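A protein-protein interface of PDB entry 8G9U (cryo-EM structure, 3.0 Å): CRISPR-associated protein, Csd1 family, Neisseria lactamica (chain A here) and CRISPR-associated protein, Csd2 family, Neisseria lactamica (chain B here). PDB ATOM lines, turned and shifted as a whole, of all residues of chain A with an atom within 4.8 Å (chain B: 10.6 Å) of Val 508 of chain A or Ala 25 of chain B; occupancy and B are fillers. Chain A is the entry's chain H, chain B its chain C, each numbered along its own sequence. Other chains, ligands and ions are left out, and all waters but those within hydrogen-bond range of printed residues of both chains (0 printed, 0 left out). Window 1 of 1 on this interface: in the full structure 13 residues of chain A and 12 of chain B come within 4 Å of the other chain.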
ATOM      1  N   ARG A 496       0.225  20.417 -16.695  1.00  0.00           N
ATOM      2  CA  ARG A 496      -0.479  19.952 -15.518  1.00  0.00           C
ATOM      3  C   ARG A 496      -1.975  19.827 -15.707  1.00  0.00           C
ATOM      4  O   ARG A 496      -2.578  18.935 -15.121  1.00  0.00           O
ATOM      5  CB  ARG A 496      -0.208  20.892 -14.342  1.00  0.00           C
ATOM      6  CG  ARG A 496      -0.466  20.263 -13.010  1.00  0.00           C
ATOM      7  CD  ARG A 496       0.434  20.867 -11.984  1.00  0.00           C
ATOM      8  NE  ARG A 496       0.300  22.311 -11.996  1.00  0.00           N
ATOM      9  CZ  ARG A 496      -0.667  22.958 -11.367  1.00  0.00           C
ATOM     10  NH1 ARG A 496      -1.567  22.278 -10.673  1.00  0.00           N
ATOM     11  NH2 ARG A 496      -0.729  24.279 -11.422  1.00  0.00           N
ATOM     12  N   TYR A 497      -2.582  20.680 -16.516  1.00  0.00           N
ATOM     13  CA  TYR A 497      -4.017  20.725 -16.686  1.00  0.00           C
ATOM     14  C   TYR A 497      -4.476  20.529 -18.114  1.00  0.00           C
ATOM     15  O   TYR A 497      -5.681  20.574 -18.351  1.00  0.00           O
ATOM     16  CB  TYR A 497      -4.576  22.072 -16.214  1.00  0.00           C
ATOM     17  CG  TYR A 497      -4.634  22.259 -14.731  1.00  0.00           C
ATOM     18  CD1 TYR A 497      -5.702  21.793 -14.000  1.00  0.00           C
ATOM     19  CD2 TYR A 497      -3.633  22.925 -14.065  1.00  0.00           C
ATOM     20  CE1 TYR A 497      -5.762  21.970 -12.649  1.00  0.00           C
ATOM     21  CE2 TYR A 497      -3.685  23.110 -12.723  1.00  0.00           C
ATOM     22  CZ  TYR A 497      -4.748  22.629 -12.012  1.00  0.00           C
ATOM     23  OH  TYR A 497      -4.799  22.813 -10.651  1.00  0.00           O
ATOM     24  N   SER A 500      -6.922  17.540 -19.478  1.00  0.00           N
ATOM     25  CA  SER A 500      -8.319  17.612 -19.110  1.00  0.00           C
ATOM     26  C   SER A 500      -8.948  18.955 -19.408  1.00  0.00           C
ATOM     27  O   SER A 500     -10.170  19.050 -19.401  1.00  0.00           O
ATOM     28  CB  SER A 500      -8.503  17.293 -17.628  1.00  0.00           C
ATOM     29  OG  SER A 500      -9.865  17.061 -17.325  1.00  0.00           O
ATOM     30  N   ALA A 501      -8.166  19.996 -19.666  1.00  0.00           N
ATOM     31  CA  ALA A 501      -8.774  21.222 -20.155  1.00  0.00           C
ATOM     32  C   ALA A 501      -9.118  21.109 -21.624  1.00  0.00           C
ATOM     33  O   ALA A 501     -10.073  21.736 -22.088  1.00  0.00           O
ATOM     34  CB  ALA A 501      -7.848  22.404 -19.928  1.00  0.00           C
ATOM     35  N   THR A 504     -12.039  18.061 -21.268  1.00  0.00           N
ATOM     36  CA  THR A 504     -12.999  18.043 -20.166  1.00  0.00           C
ATOM     37  C   THR A 504     -12.958  19.377 -19.438  1.00  0.00           C
ATOM     38  O   THR A 504     -12.482  19.481 -18.304  1.00  0.00           O
ATOM     39  CB  THR A 504     -12.688  16.892 -19.224  1.00  0.00           C
ATOM     40  OG1 THR A 504     -12.727  15.664 -19.954  1.00  0.00           O
ATOM     41  CG2 THR A 504     -13.696  16.835 -18.190  1.00  0.00           C
ATOM     42  N   PRO A 505     -13.446  20.431 -20.074  1.00  0.00           N
ATOM     43  CA  PRO A 505     -13.198  21.769 -19.542  1.00  0.00           C
ATOM     44  C   PRO A 505     -13.775  22.056 -18.171  1.00  0.00           C
ATOM     45  O   PRO A 505     -13.195  22.869 -17.455  1.00  0.00           O
ATOM     46  CB  PRO A 505     -13.825  22.650 -20.608  1.00  0.00           C
ATOM     47  CG  PRO A 505     -13.639  21.886 -21.828  1.00  0.00           C
ATOM     48  CD  PRO A 505     -13.979  20.500 -21.435  1.00  0.00           C
ATOM     49  N   ILE A 506     -14.904  21.473 -17.772  1.00  0.00           N
ATOM     50  CA  ILE A 506     -15.367  21.812 -16.431  1.00  0.00           C
ATOM     51  C   ILE A 506     -14.452  21.202 -15.389  1.00  0.00           C
ATOM     52  O   ILE A 506     -14.294  21.754 -14.296  1.00  0.00           O
ATOM     53  CB  ILE A 506     -16.815  21.384 -16.180  1.00  0.00           C
ATOM     54  CG1 ILE A 506     -16.983  19.896 -16.415  1.00  0.00           C
ATOM     55  CG2 ILE A 506     -17.750  22.173 -17.016  1.00  0.00           C
ATOM     56  CD1 ILE A 506     -18.153  19.345 -15.672  1.00  0.00           C
ATOM     57  N   ALA A 507     -13.848  20.058 -15.691  1.00  0.00           N
ATOM     58  CA  ALA A 507     -12.952  19.445 -14.728  1.00  0.00           C
ATOM     59  C   ALA A 507     -11.801  20.357 -14.374  1.00  0.00           C
ATOM     60  O   ALA A 507     -11.247  20.242 -13.279  1.00  0.00           O
ATOM     61  CB  ALA A 507     -12.402  18.131 -15.268  1.00  0.00           C
ATOM     62  N   VAL A 508     -11.443  21.273 -15.261  1.00  0.00           N
ATOM     63  CA  VAL A 508     -10.188  21.984 -15.121  1.00  0.00           C
ATOM     64  C   VAL A 508     -10.421  23.480 -15.066  1.00  0.00           C
ATOM     65  O   VAL A 508     -10.095  24.124 -14.071  1.00  0.00           O
ATOM     66  CB  VAL A 508      -9.246  21.611 -16.267  1.00  0.00           C
ATOM     67  CG1 VAL A 508      -8.176  22.609 -16.391  1.00  0.00           C
ATOM     68  CG2 VAL A 508      -8.646  20.291 -15.990  1.00  0.00           C
ATOM     69  N   PHE A 509     -11.000  24.045 -16.121  1.00  0.00           N
ATOM     70  CA  PHE A 509     -11.148  25.488 -16.236  1.00  0.00           C
ATOM     71  C   PHE A 509     -11.876  26.112 -15.066  1.00  0.00           C
ATOM     72  O   PHE A 509     -11.800  27.329 -14.891  1.00  0.00           O
ATOM     73  CB  PHE A 509     -11.874  25.831 -17.520  1.00  0.00           C
ATOM     74  CG  PHE A 509     -10.998  25.795 -18.705  1.00  0.00           C
ATOM     75  CD1 PHE A 509      -9.951  26.667 -18.812  1.00  0.00           C
ATOM     76  CD2 PHE A 509     -11.201  24.878 -19.698  1.00  0.00           C
ATOM     77  CE1 PHE A 509      -9.135  26.636 -19.895  1.00  0.00           C
ATOM     78  CE2 PHE A 509     -10.384  24.844 -20.784  1.00  0.00           C
ATOM     79  CZ  PHE A 509      -9.349  25.724 -20.883  1.00  0.00           C
ATOM     80  N   GLY A 510     -12.575  25.321 -14.263  1.00  0.00           N
ATOM     81  CA  GLY A 510     -13.040  25.842 -13.002  1.00  0.00           C
ATOM     82  C   GLY A 510     -11.939  25.996 -11.981  1.00  0.00           C
ATOM     83  O   GLY A 510     -12.162  26.623 -10.947  1.00  0.00           O
ATOM     84  N   THR A 511     -10.762  25.425 -12.240  1.00  0.00           N
ATOM     85  CA  THR A 511      -9.651  25.469 -11.303  1.00  0.00           C
ATOM     86  C   THR A 511      -8.410  26.107 -11.887  1.00  0.00           C
ATOM     87  O   THR A 511      -7.548  26.557 -11.130  1.00  0.00           O
ATOM     88  CB  THR A 511      -9.286  24.062 -10.843  1.00  0.00           C
ATOM     89  OG1 THR A 511      -8.493  23.438 -11.851  1.00  0.00           O
ATOM     90  CG2 THR A 511     -10.547  23.256 -10.679  1.00  0.00           C
ATOM     91  N   LEU A 512      -8.282  26.108 -13.207  1.00  0.00           N
ATOM     92  CA  LEU A 512      -7.290  26.940 -13.865  1.00  0.00           C
ATOM     93  C   LEU A 512      -7.511  28.391 -13.525  1.00  0.00           C
ATOM     94  O   LEU A 512      -6.560  29.162 -13.374  1.00  0.00           O
ATOM     95  CB  LEU A 512      -7.381  26.767 -15.367  1.00  0.00           C
ATOM     96  CG  LEU A 512      -6.658  25.565 -15.897  1.00  0.00           C
ATOM     97  CD1 LEU A 512      -6.661  25.653 -17.377  1.00  0.00           C
ATOM     98  CD2 LEU A 512      -5.277  25.586 -15.369  1.00  0.00           C
ATOM     99  N   ASN B  18      -7.706  13.501  -1.807  1.00  0.00           N
ATOM    100  CA  ASN B  18      -7.669  13.246  -3.230  1.00  0.00           C
ATOM    101  C   ASN B  18      -7.629  11.749  -3.468  1.00  0.00           C
ATOM    102  O   ASN B  18      -6.558  11.141  -3.382  1.00  0.00           O
ATOM    103  CB  ASN B  18      -6.442  13.914  -3.830  1.00  0.00           C
ATOM    104  CG  ASN B  18      -6.572  14.143  -5.290  1.00  0.00           C
ATOM    105  OD1 ASN B  18      -7.362  13.497  -5.957  1.00  0.00           O
ATOM    106  ND2 ASN B  18      -5.782  15.061  -5.811  1.00  0.00           N
ATOM    107  N   ASN B  20      -8.015   9.952  -6.221  1.00  0.00           N
ATOM    108  CA  ASN B  20      -7.237   9.651  -7.410  1.00  0.00           C
ATOM    109  C   ASN B  20      -7.158  10.946  -8.205  1.00  0.00           C
ATOM    110  O   ASN B  20      -8.113  11.299  -8.894  1.00  0.00           O
ATOM    111  CB  ASN B  20      -7.884   8.552  -8.218  1.00  0.00           C
ATOM    112  CG  ASN B  20      -6.986   8.036  -9.278  1.00  0.00           C
ATOM    113  OD1 ASN B  20      -7.276   8.143 -10.463  1.00  0.00           O
ATOM    114  ND2 ASN B  20      -5.871   7.470  -8.868  1.00  0.00           N
ATOM    115  N   GLY B  21      -6.037  11.644  -8.095  1.00  0.00           N
ATOM    116  CA  GLY B  21      -5.886  12.876  -8.831  1.00  0.00           C
ATOM    117  C   GLY B  21      -5.830  12.612 -10.319  1.00  0.00           C
ATOM    118  O   GLY B  21      -5.276  11.615 -10.771  1.00  0.00           O
ATOM    119  N   ASP B  22      -6.428  13.510 -11.088  1.00  0.00           N
ATOM    120  CA  ASP B  22      -6.381  13.409 -12.534  1.00  0.00           C
ATOM    121  C   ASP B  22      -5.144  14.146 -13.006  1.00  0.00           C
ATOM    122  O   ASP B  22      -5.121  15.380 -12.957  1.00  0.00           O
ATOM    123  CB  ASP B  22      -7.627  14.011 -13.161  1.00  0.00           C
ATOM    124  CG  ASP B  22      -7.978  13.380 -14.502  1.00  0.00           C
ATOM    125  OD1 ASP B  22      -7.214  12.523 -14.985  1.00  0.00           O
ATOM    126  OD2 ASP B  22      -9.025  13.745 -15.074  1.00  0.00           O
ATOM    127  N   PRO B  23      -4.105  13.455 -13.455  1.00  0.00           N
ATOM    128  CA  PRO B  23      -2.937  14.169 -13.973  1.00  0.00           C
ATOM    129  C   PRO B  23      -3.283  15.108 -15.094  1.00  0.00           C
ATOM    130  O   PRO B  23      -2.637  16.145 -15.266  1.00  0.00           O
ATOM    131  CB  PRO B  23      -2.046  13.036 -14.458  1.00  0.00           C
ATOM    132  CG  PRO B  23      -2.421  11.905 -13.638  1.00  0.00           C
ATOM    133  CD  PRO B  23      -3.881  12.010 -13.421  1.00  0.00           C
ATOM    134  N   ASP B  24      -4.287  14.750 -15.880  1.00  0.00           N
ATOM    135  CA  ASP B  24      -4.828  15.662 -16.863  1.00  0.00           C
ATOM    136  C   ASP B  24      -5.423  16.898 -16.222  1.00  0.00           C
ATOM    137  O   ASP B  24      -5.488  17.941 -16.870  1.00  0.00           O
ATOM    138  CB  ASP B  24      -5.891  14.950 -17.682  1.00  0.00           C
ATOM    139  CG  ASP B  24      -5.304  14.135 -18.792  1.00  0.00           C
ATOM    140  OD1 ASP B  24      -4.082  14.248 -19.024  1.00  0.00           O
ATOM    141  OD2 ASP B  24      -6.054  13.375 -19.438  1.00  0.00           O
ATOM    142  N   ALA B  25      -5.871  16.806 -14.977  1.00  0.00           N
ATOM    143  CA  ALA B  25      -6.507  17.926 -14.296  1.00  0.00           C
ATOM    144  C   ALA B  25      -5.692  18.239 -13.056  1.00  0.00           C
ATOM    145  O   ALA B  25      -6.053  17.848 -11.948  1.00  0.00           O
ATOM    146  CB  ALA B  25      -7.908  17.585 -13.954  1.00  0.00           C
ATOM    147  N   GLY B  26      -4.610  18.982 -13.243  1.00  0.00           N
ATOM    148  CA  GLY B  26      -3.736  19.303 -12.140  1.00  0.00           C
ATOM    149  C   GLY B  26      -3.411  18.059 -11.358  1.00  0.00           C
ATOM    150  O   GLY B  26      -2.701  17.170 -11.824  1.00  0.00           O
ATOM    151  N   ASN B  27      -3.937  18.003 -10.156  1.00  0.00           N
ATOM    152  CA  ASN B  27      -4.028  16.751  -9.430  1.00  0.00           C
ATOM    153  C   ASN B  27      -5.410  16.611  -8.823  1.00  0.00           C
ATOM    154  O   ASN B  27      -5.598  15.782  -7.932  1.00  0.00           O
ATOM    155  CB  ASN B  27      -2.961  16.666  -8.346  1.00  0.00           C
ATOM    156  CG  ASN B  27      -2.830  15.289  -7.779  1.00  0.00           C
ATOM    157  OD1 ASN B  27      -3.023  14.311  -8.480  1.00  0.00           O
ATOM    158  ND2 ASN B  27      -2.523  15.198  -6.494  1.00  0.00           N
ATOM    159  N   LEU B  28      -6.370  17.413  -9.257  1.00  0.00           N
ATOM    160  CA  LEU B  28      -7.679  17.373  -8.651  1.00  0.00           C
ATOM    161  C   LEU B  28      -8.344  16.047  -8.982  1.00  0.00           C
ATOM    162  O   LEU B  28      -8.130  15.497 -10.060  1.00  0.00           O
ATOM    163  CB  LEU B  28      -8.512  18.559  -9.120  1.00  0.00           C
ATOM    164  CG  LEU B  28      -8.840  18.728 -10.593  1.00  0.00           C
ATOM    165  CD1 LEU B  28     -10.051  17.917 -11.034  1.00  0.00           C
ATOM    166  CD2 LEU B  28      -9.023  20.181 -10.878  1.00  0.00           C
ATOM    167  N   PRO B  29      -9.135  15.509  -8.059  1.00  0.00           N
ATOM    168  CA  PRO B  29      -9.549  14.114  -8.166  1.00  0.00           C
ATOM    169  C   PRO B  29     -10.249  13.853  -9.479  1.00  0.00           C
ATOM    170  O   PRO B  29     -10.870  14.740 -10.057  1.00  0.00           O
ATOM    171  CB  PRO B  29     -10.502  13.940  -6.985  1.00  0.00           C
ATOM    172  CG  PRO B  29     -10.098  14.972  -6.040  1.00  0.00           C
ATOM    173  CD  PRO B  29      -9.632  16.127  -6.828  1.00  0.00           C
ATOM    174  N   ARG B  30     -10.080  12.642  -9.986  1.00  0.00           N
ATOM    175  CA  ARG B  30     -10.796  12.276 -11.188  1.00  0.00           C
ATOM    176  C   ARG B  30     -12.281  12.403 -10.940  1.00  0.00           C
ATOM    177  O   ARG B  30     -12.788  12.042  -9.879  1.00  0.00           O
ATOM    178  CB  ARG B  30     -10.463  10.864 -11.614  1.00  0.00           C
ATOM    179  CG  ARG B  30      -9.042  10.683 -11.927  1.00  0.00           C
ATOM    180  CD  ARG B  30      -8.879   9.480 -12.752  1.00  0.00           C
ATOM    181  NE  ARG B  30      -7.511   9.026 -12.702  1.00  0.00           N
ATOM    182  CZ  ARG B  30      -6.594   9.411 -13.567  1.00  0.00           C
ATOM    183  NH1 ARG B  30      -6.911  10.262 -14.521  1.00  0.00           N
ATOM    184  NH2 ARG B  30      -5.365   8.954 -13.474  1.00  0.00           N
ATOM    185  N   ILE B  31     -12.967  12.941 -11.926  1.00  0.00           N
ATOM    186  CA  ILE B  31     -14.370  13.294 -11.825  1.00  0.00           C
ATOM    187  C   ILE B  31     -15.070  12.931 -13.118  1.00  0.00           C
ATOM    188  O   ILE B  31     -14.530  13.125 -14.211  1.00  0.00           O
ATOM    189  CB  ILE B  31     -14.510  14.785 -11.474  1.00  0.00           C
ATOM    190  CG1 ILE B  31     -14.015  15.613 -12.642  1.00  0.00           C
ATOM    191  CG2 ILE B  31     -13.869  15.135 -10.169  1.00  0.00           C
ATOM    192  CD1 ILE B  31     -14.283  17.008 -12.506  1.00  0.00           C
ATOM    193  N   ASP B  32     -16.235  12.341 -12.988  1.00  0.00           N
ATOM    194  CA  ASP B  32     -17.129  12.230 -14.120  1.00  0.00           C
ATOM    195  C   ASP B  32     -17.729  13.608 -14.319  1.00  0.00           C
ATOM    196  O   ASP B  32     -18.640  14.006 -13.587  1.00  0.00           O
ATOM    197  CB  ASP B  32     -18.209  11.194 -13.866  1.00  0.00           C
ATOM    198  CG  ASP B  32     -18.827  10.694 -15.127  1.00  0.00           C
ATOM    199  OD1 ASP B  32     -19.158  11.521 -15.997  1.00  0.00           O
ATOM    200  OD2 ASP B  32     -19.028   9.473 -15.236  1.00  0.00           O
ATOM    201  N   PRO B  33     -17.269  14.331 -15.290  1.00  0.00           N
ATOM    202  CA  PRO B  33     -17.564  15.762 -15.373  1.00  0.00           C
ATOM    203  C   PRO B  33     -19.037  16.061 -15.544  1.00  0.00           C
ATOM    204  O   PRO B  33     -19.633  16.763 -14.725  1.00  0.00           O
ATOM    205  CB  PRO B  33     -16.768  16.201 -16.602  1.00  0.00           C
ATOM    206  CG  PRO B  33     -15.998  14.999 -17.006  1.00  0.00           C
ATOM    207  CD  PRO B  33     -16.664  13.828 -16.514  1.00  0.00           C
ATOM    208  N   GLN B  34     -19.646  15.512 -16.591  1.00  0.00           N
ATOM    209  CA  GLN B  34     -21.046  15.807 -16.852  1.00  0.00           C
ATOM    210  C   GLN B  34     -21.975  15.328 -15.753  1.00  0.00           C
ATOM    211  O   GLN B  34     -23.164  15.659 -15.793  1.00  0.00           O
ATOM    212  CB  GLN B  34     -21.457  15.231 -18.204  1.00  0.00           C
ATOM    213  CG  GLN B  34     -21.501  13.739 -18.252  1.00  0.00           C
ATOM    214  CD  GLN B  34     -20.139  13.174 -18.542  1.00  0.00           C
ATOM    215  OE1 GLN B  34     -19.135  13.864 -18.407  1.00  0.00           O
ATOM    216  NE2 GLN B  34     -20.092  11.931 -18.969  1.00  0.00           N
ATOM    217  N   LEU B  39     -14.196   9.974  -9.759  1.00  0.00           N
ATOM    218  CA  LEU B  39     -13.702   8.740 -10.335  1.00  0.00           C
ATOM    219  C   LEU B  39     -12.399   8.374  -9.659  1.00  0.00           C
ATOM    220  O   LEU B  39     -11.637   9.237  -9.230  1.00  0.00           O
ATOM    221  CB  LEU B  39     -13.487   8.854 -11.833  1.00  0.00           C
ATOM    222  CG  LEU B  39     -14.788   8.928 -12.604  1.00  0.00           C
ATOM    223  CD1 LEU B  39     -14.550   9.616 -13.904  1.00  0.00           C
ATOM    224  CD2 LEU B  39     -15.309   7.542 -12.825  1.00  0.00           C
ATOM    225  N   ILE B 139     -18.568  14.328  -6.068  1.00  0.00           N
ATOM    226  CA  ILE B 139     -17.559  14.780  -5.130  1.00  0.00           C
ATOM    227  C   ILE B 139     -17.399  16.282  -5.282  1.00  0.00           C
ATOM    228  O   ILE B 139     -17.310  16.810  -6.397  1.00  0.00           O
ATOM    229  CB  ILE B 139     -16.235  14.043  -5.356  1.00  0.00           C
ATOM    230  CG1 ILE B 139     -15.669  14.357  -6.730  1.00  0.00           C
ATOM    231  CG2 ILE B 139     -16.440  12.566  -5.218  1.00  0.00           C
ATOM    232  CD1 ILE B 139     -14.226  14.081  -6.841  1.00  0.00           C
ATOM    233  N   THR B 141     -14.955  18.411  -4.855  1.00  0.00           N
ATOM    234  CA  THR B 141     -13.518  18.596  -4.708  1.00  0.00           C
ATOM    235  C   THR B 141     -13.200  19.978  -4.174  1.00  0.00           C
ATOM    236  O   THR B 141     -13.521  20.989  -4.804  1.00  0.00           O
ATOM    237  CB  THR B 141     -12.834  18.386  -6.050  1.00  0.00           C
ATOM    238  OG1 THR B 141     -12.771  16.989  -6.339  1.00  0.00           O
ATOM    239  CG2 THR B 141     -11.445  18.925  -6.001  1.00  0.00           C
ATOM    240  N   GLU B 143     -10.200  21.507  -3.255  1.00  0.00           N
ATOM    241  CA  GLU B 143      -9.052  22.248  -3.765  1.00  0.00           C
ATOM    242  C   GLU B 143      -8.542  23.225  -2.715  1.00  0.00           C
ATOM    243  O   GLU B 143      -8.586  24.442  -2.880  1.00  0.00           O
ATOM    244  CB  GLU B 143      -9.396  22.974  -5.060  1.00  0.00           C
ATOM    245  CG  GLU B 143     -10.120  22.102  -6.027  1.00  0.00           C
ATOM    246  CD  GLU B 143     -10.479  22.830  -7.269  1.00  0.00           C
ATOM    247  OE1 GLU B 143      -9.634  23.614  -7.737  1.00  0.00           O
ATOM    248  OE2 GLU B 143     -11.604  22.635  -7.775  1.00  0.00           O
ATOM    249  N   ARG B 168      -1.247  23.652  -4.024  1.00  0.00           N
ATOM    250  CA  ARG B 168      -2.661  23.356  -3.922  1.00  0.00           C
ATOM    251  C   ARG B 168      -2.849  21.911  -3.498  1.00  0.00           C
ATOM    252  O   ARG B 168      -2.119  21.021  -3.932  1.00  0.00           O
ATOM    253  CB  ARG B 168      -3.354  23.626  -5.255  1.00  0.00           C
ATOM    254  CG  ARG B 168      -4.826  23.401  -5.248  1.00  0.00           C
ATOM    255  CD  ARG B 168      -5.517  24.373  -4.345  1.00  0.00           C
ATOM    256  NE  ARG B 168      -5.299  25.753  -4.743  1.00  0.00           N
ATOM    257  CZ  ARG B 168      -6.021  26.377  -5.660  1.00  0.00           C
ATOM    258  NH1 ARG B 168      -5.759  27.635  -5.966  1.00  0.00           N
ATOM    259  NH2 ARG B 168      -7.019  25.745  -6.258  1.00  0.00           N
ATOM    260  N   LYS B 169      -3.835  21.690  -2.641  1.00  0.00           N
ATOM    261  CA  LYS B 169      -4.130  20.376  -2.082  1.00  0.00           C
ATOM    262  C   LYS B 169      -5.601  20.101  -2.341  1.00  0.00           C
ATOM    263  O   LYS B 169      -6.461  20.581  -1.601  1.00  0.00           O
ATOM    264  CB  LYS B 169      -3.822  20.327  -0.596  1.00  0.00           C
ATOM    265  CG  LYS B 169      -4.161  19.020   0.069  1.00  0.00           C
ATOM    266  CD  LYS B 169      -2.949  18.139   0.160  1.00  0.00           C
ATOM    267  CE  LYS B 169      -2.028  18.621   1.240  1.00  0.00           C
ATOM    268  NZ  LYS B 169      -0.709  17.950   1.157  1.00  0.00           N
ATOM    269  N   PHE B 170      -5.892  19.341  -3.384  1.00  0.00           N
ATOM    270  CA  PHE B 170      -7.267  19.015  -3.720  1.00  0.00           C
ATOM    271  C   PHE B 170      -7.750  17.912  -2.802  1.00  0.00           C
ATOM    272  O   PHE B 170      -7.093  16.878  -2.679  1.00  0.00           O
ATOM    273  CB  PHE B 170      -7.364  18.575  -5.170  1.00  0.00           C
ATOM    274  CG  PHE B 170      -6.613  19.445  -6.104  1.00  0.00           C
ATOM    275  CD1 PHE B 170      -7.157  20.622  -6.542  1.00  0.00           C
ATOM    276  CD2 PHE B 170      -5.357  19.095  -6.536  1.00  0.00           C
ATOM    277  CE1 PHE B 170      -6.476  21.426  -7.408  1.00  0.00           C
ATOM    278  CE2 PHE B 170      -4.666  19.900  -7.400  1.00  0.00           C
ATOM    279  CZ  PHE B 170      -5.225  21.069  -7.836  1.00  0.00           C
ATOM    280  N   THR B 171      -8.876  18.132  -2.145  1.00  0.00           N
ATOM    281  CA  THR B 171      -9.467  17.117  -1.294  1.00  0.00           C
ATOM    282  C   THR B 171     -10.932  16.961  -1.636  1.00  0.00           C
ATOM    283  O   THR B 171     -11.624  17.944  -1.903  1.00  0.00           O
ATOM    284  CB  THR B 171      -9.350  17.452   0.187  1.00  0.00           C
ATOM    285  OG1 THR B 171     -10.312  18.453   0.527  1.00  0.00           O
ATOM    286  CG2 THR B 171      -7.969  17.950   0.509  1.00  0.00           C
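O of Tyr 497 of chain A sits close to O of Asp 24 of chain B (3.0 Å).
The backbone carbonyl oxygen (O) of Arg 496 of chain A lies close to the backbone carbonyl oxygen (O) of Pro 23 of chain B (2.8 Å).
The backbone carbonyl oxygen (O) of Arg 496 of chain A lies within hydrogen-bond range of the backbone NH (N) of Gly 26 of chain B (2.8 Å).
N of Ser 500 of chain A sits at hydrogen-bond distance from O of Asp 24 of chain B (3.0 Å).
Ala 25 of chain B touches Arg 496 of chain A (C to O, 3.8 Å).
Ala 25 of chain B touches Tyr 497 of chain A.
OH of Tyr 497 of chain A touches CZ of Phe 170 of chain B, at 3.3 Å.
Ala 25 of chain B touches Ser 500 of chain A (CB to CB, 3.7 Å).
Thr 504 of chain A touches Pro 33 of chain B.
O of Pro 33 of chain B touches CD1 of Ile 506 of chain A, at 3.1 Å.
Ala 507 of chain A touches Ile 31 of chain B (CB to CD1, 3.5 Å).
CB of Ala 25 of chain B touches CG2 of Val 508 of chain A (3.5 Å).
Thr 511 of chain A touches Leu 28 of chain B (CG2 to CD2, 3.4 Å).
Thr 511 of chain A touches Glu 143 of chain B.
The side-chain hydroxyl (OG1) of Thr 511 of chain A lies within hydrogen-bond range of the backbone carbonyl oxygen (O) of Val 508 of chain A (2.8 Å).
The backbone NH (N) of Asp 22 of chain B lies within hydrogen-bond range of the backbone carbonyl oxygen (O) of Leu 28 of chain B.
The side-chain hydroxyl (OH) of Tyr 497 of chain A sits close to the guanidinium group (NH1) of Arg 496 of chain A, at 3.3 Å.
OE1 of Glu 143 of chain B lies within salt-bridge range of NH2 of Arg 168 of chain B (3.7 Å).
Of chain B, only Ala 25 (3.5 Å) comes within 4 Å of Val 508 of chain A.
Of chain B, only Asp 24 (3.0 Å), Ala 25 (3.7 Å), Gly 26 (3.1 Å) and Phe 170 (3.3 Å) come within 4 Å of Tyr 497 of chain A.
No residue of chain B comes within 4 Å of Ala 501 of chain A.
Of the printed residues of chain B, Ala 507 of chain A touches Leu 28 and Ile 31.
No residue of chain B comes within 4 Å of Phe 509 of chain A.
No residue of chain B comes within 4 Å of Gly 510 of chain A.
Of the printed residues of chain B, Thr 511 of chain A touches Leu 28 and Glu 143.
No residue of chain B comes within 4 Å of Leu 512 of chain A.
Printed residues of chain A within 4 Å of Phe 170 of chain B: Tyr 497.
Printed residues of chain A within 4 Å of Pro 33 of chain B: Thr 504 (3.2 Å) and Ile 506 (3.1 Å).
Printed residues of chain A within 4 Å of Pro 23 of chain B: Arg 496 (2.8 Å).
Of the printed residues of chain A, Ile 31 of chain B touches Ala 507.
Of the printed residues of chain A, Gly 26 of chain B touches Arg 496 and Tyr 497.
Leu 39 of chain B touches none of the printed residues of chain A.
Of the 24 printed residues of chain B, 9 touch a printed residue of chain A.
Hydrophobic or aromatic side chains of chain B within 4 Å of the printed part of chain A: Ala 25, Leu 28, Ile 31, Pro 33 and Phe 170.
Of the 13 printed residues of chain A, 8 touch a printed residue of chain B.
Among the printed residues, no Asp or Glu carboxylate lies within 4 Å of a Lys or Arg side-chain nitrogen of the other chain.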
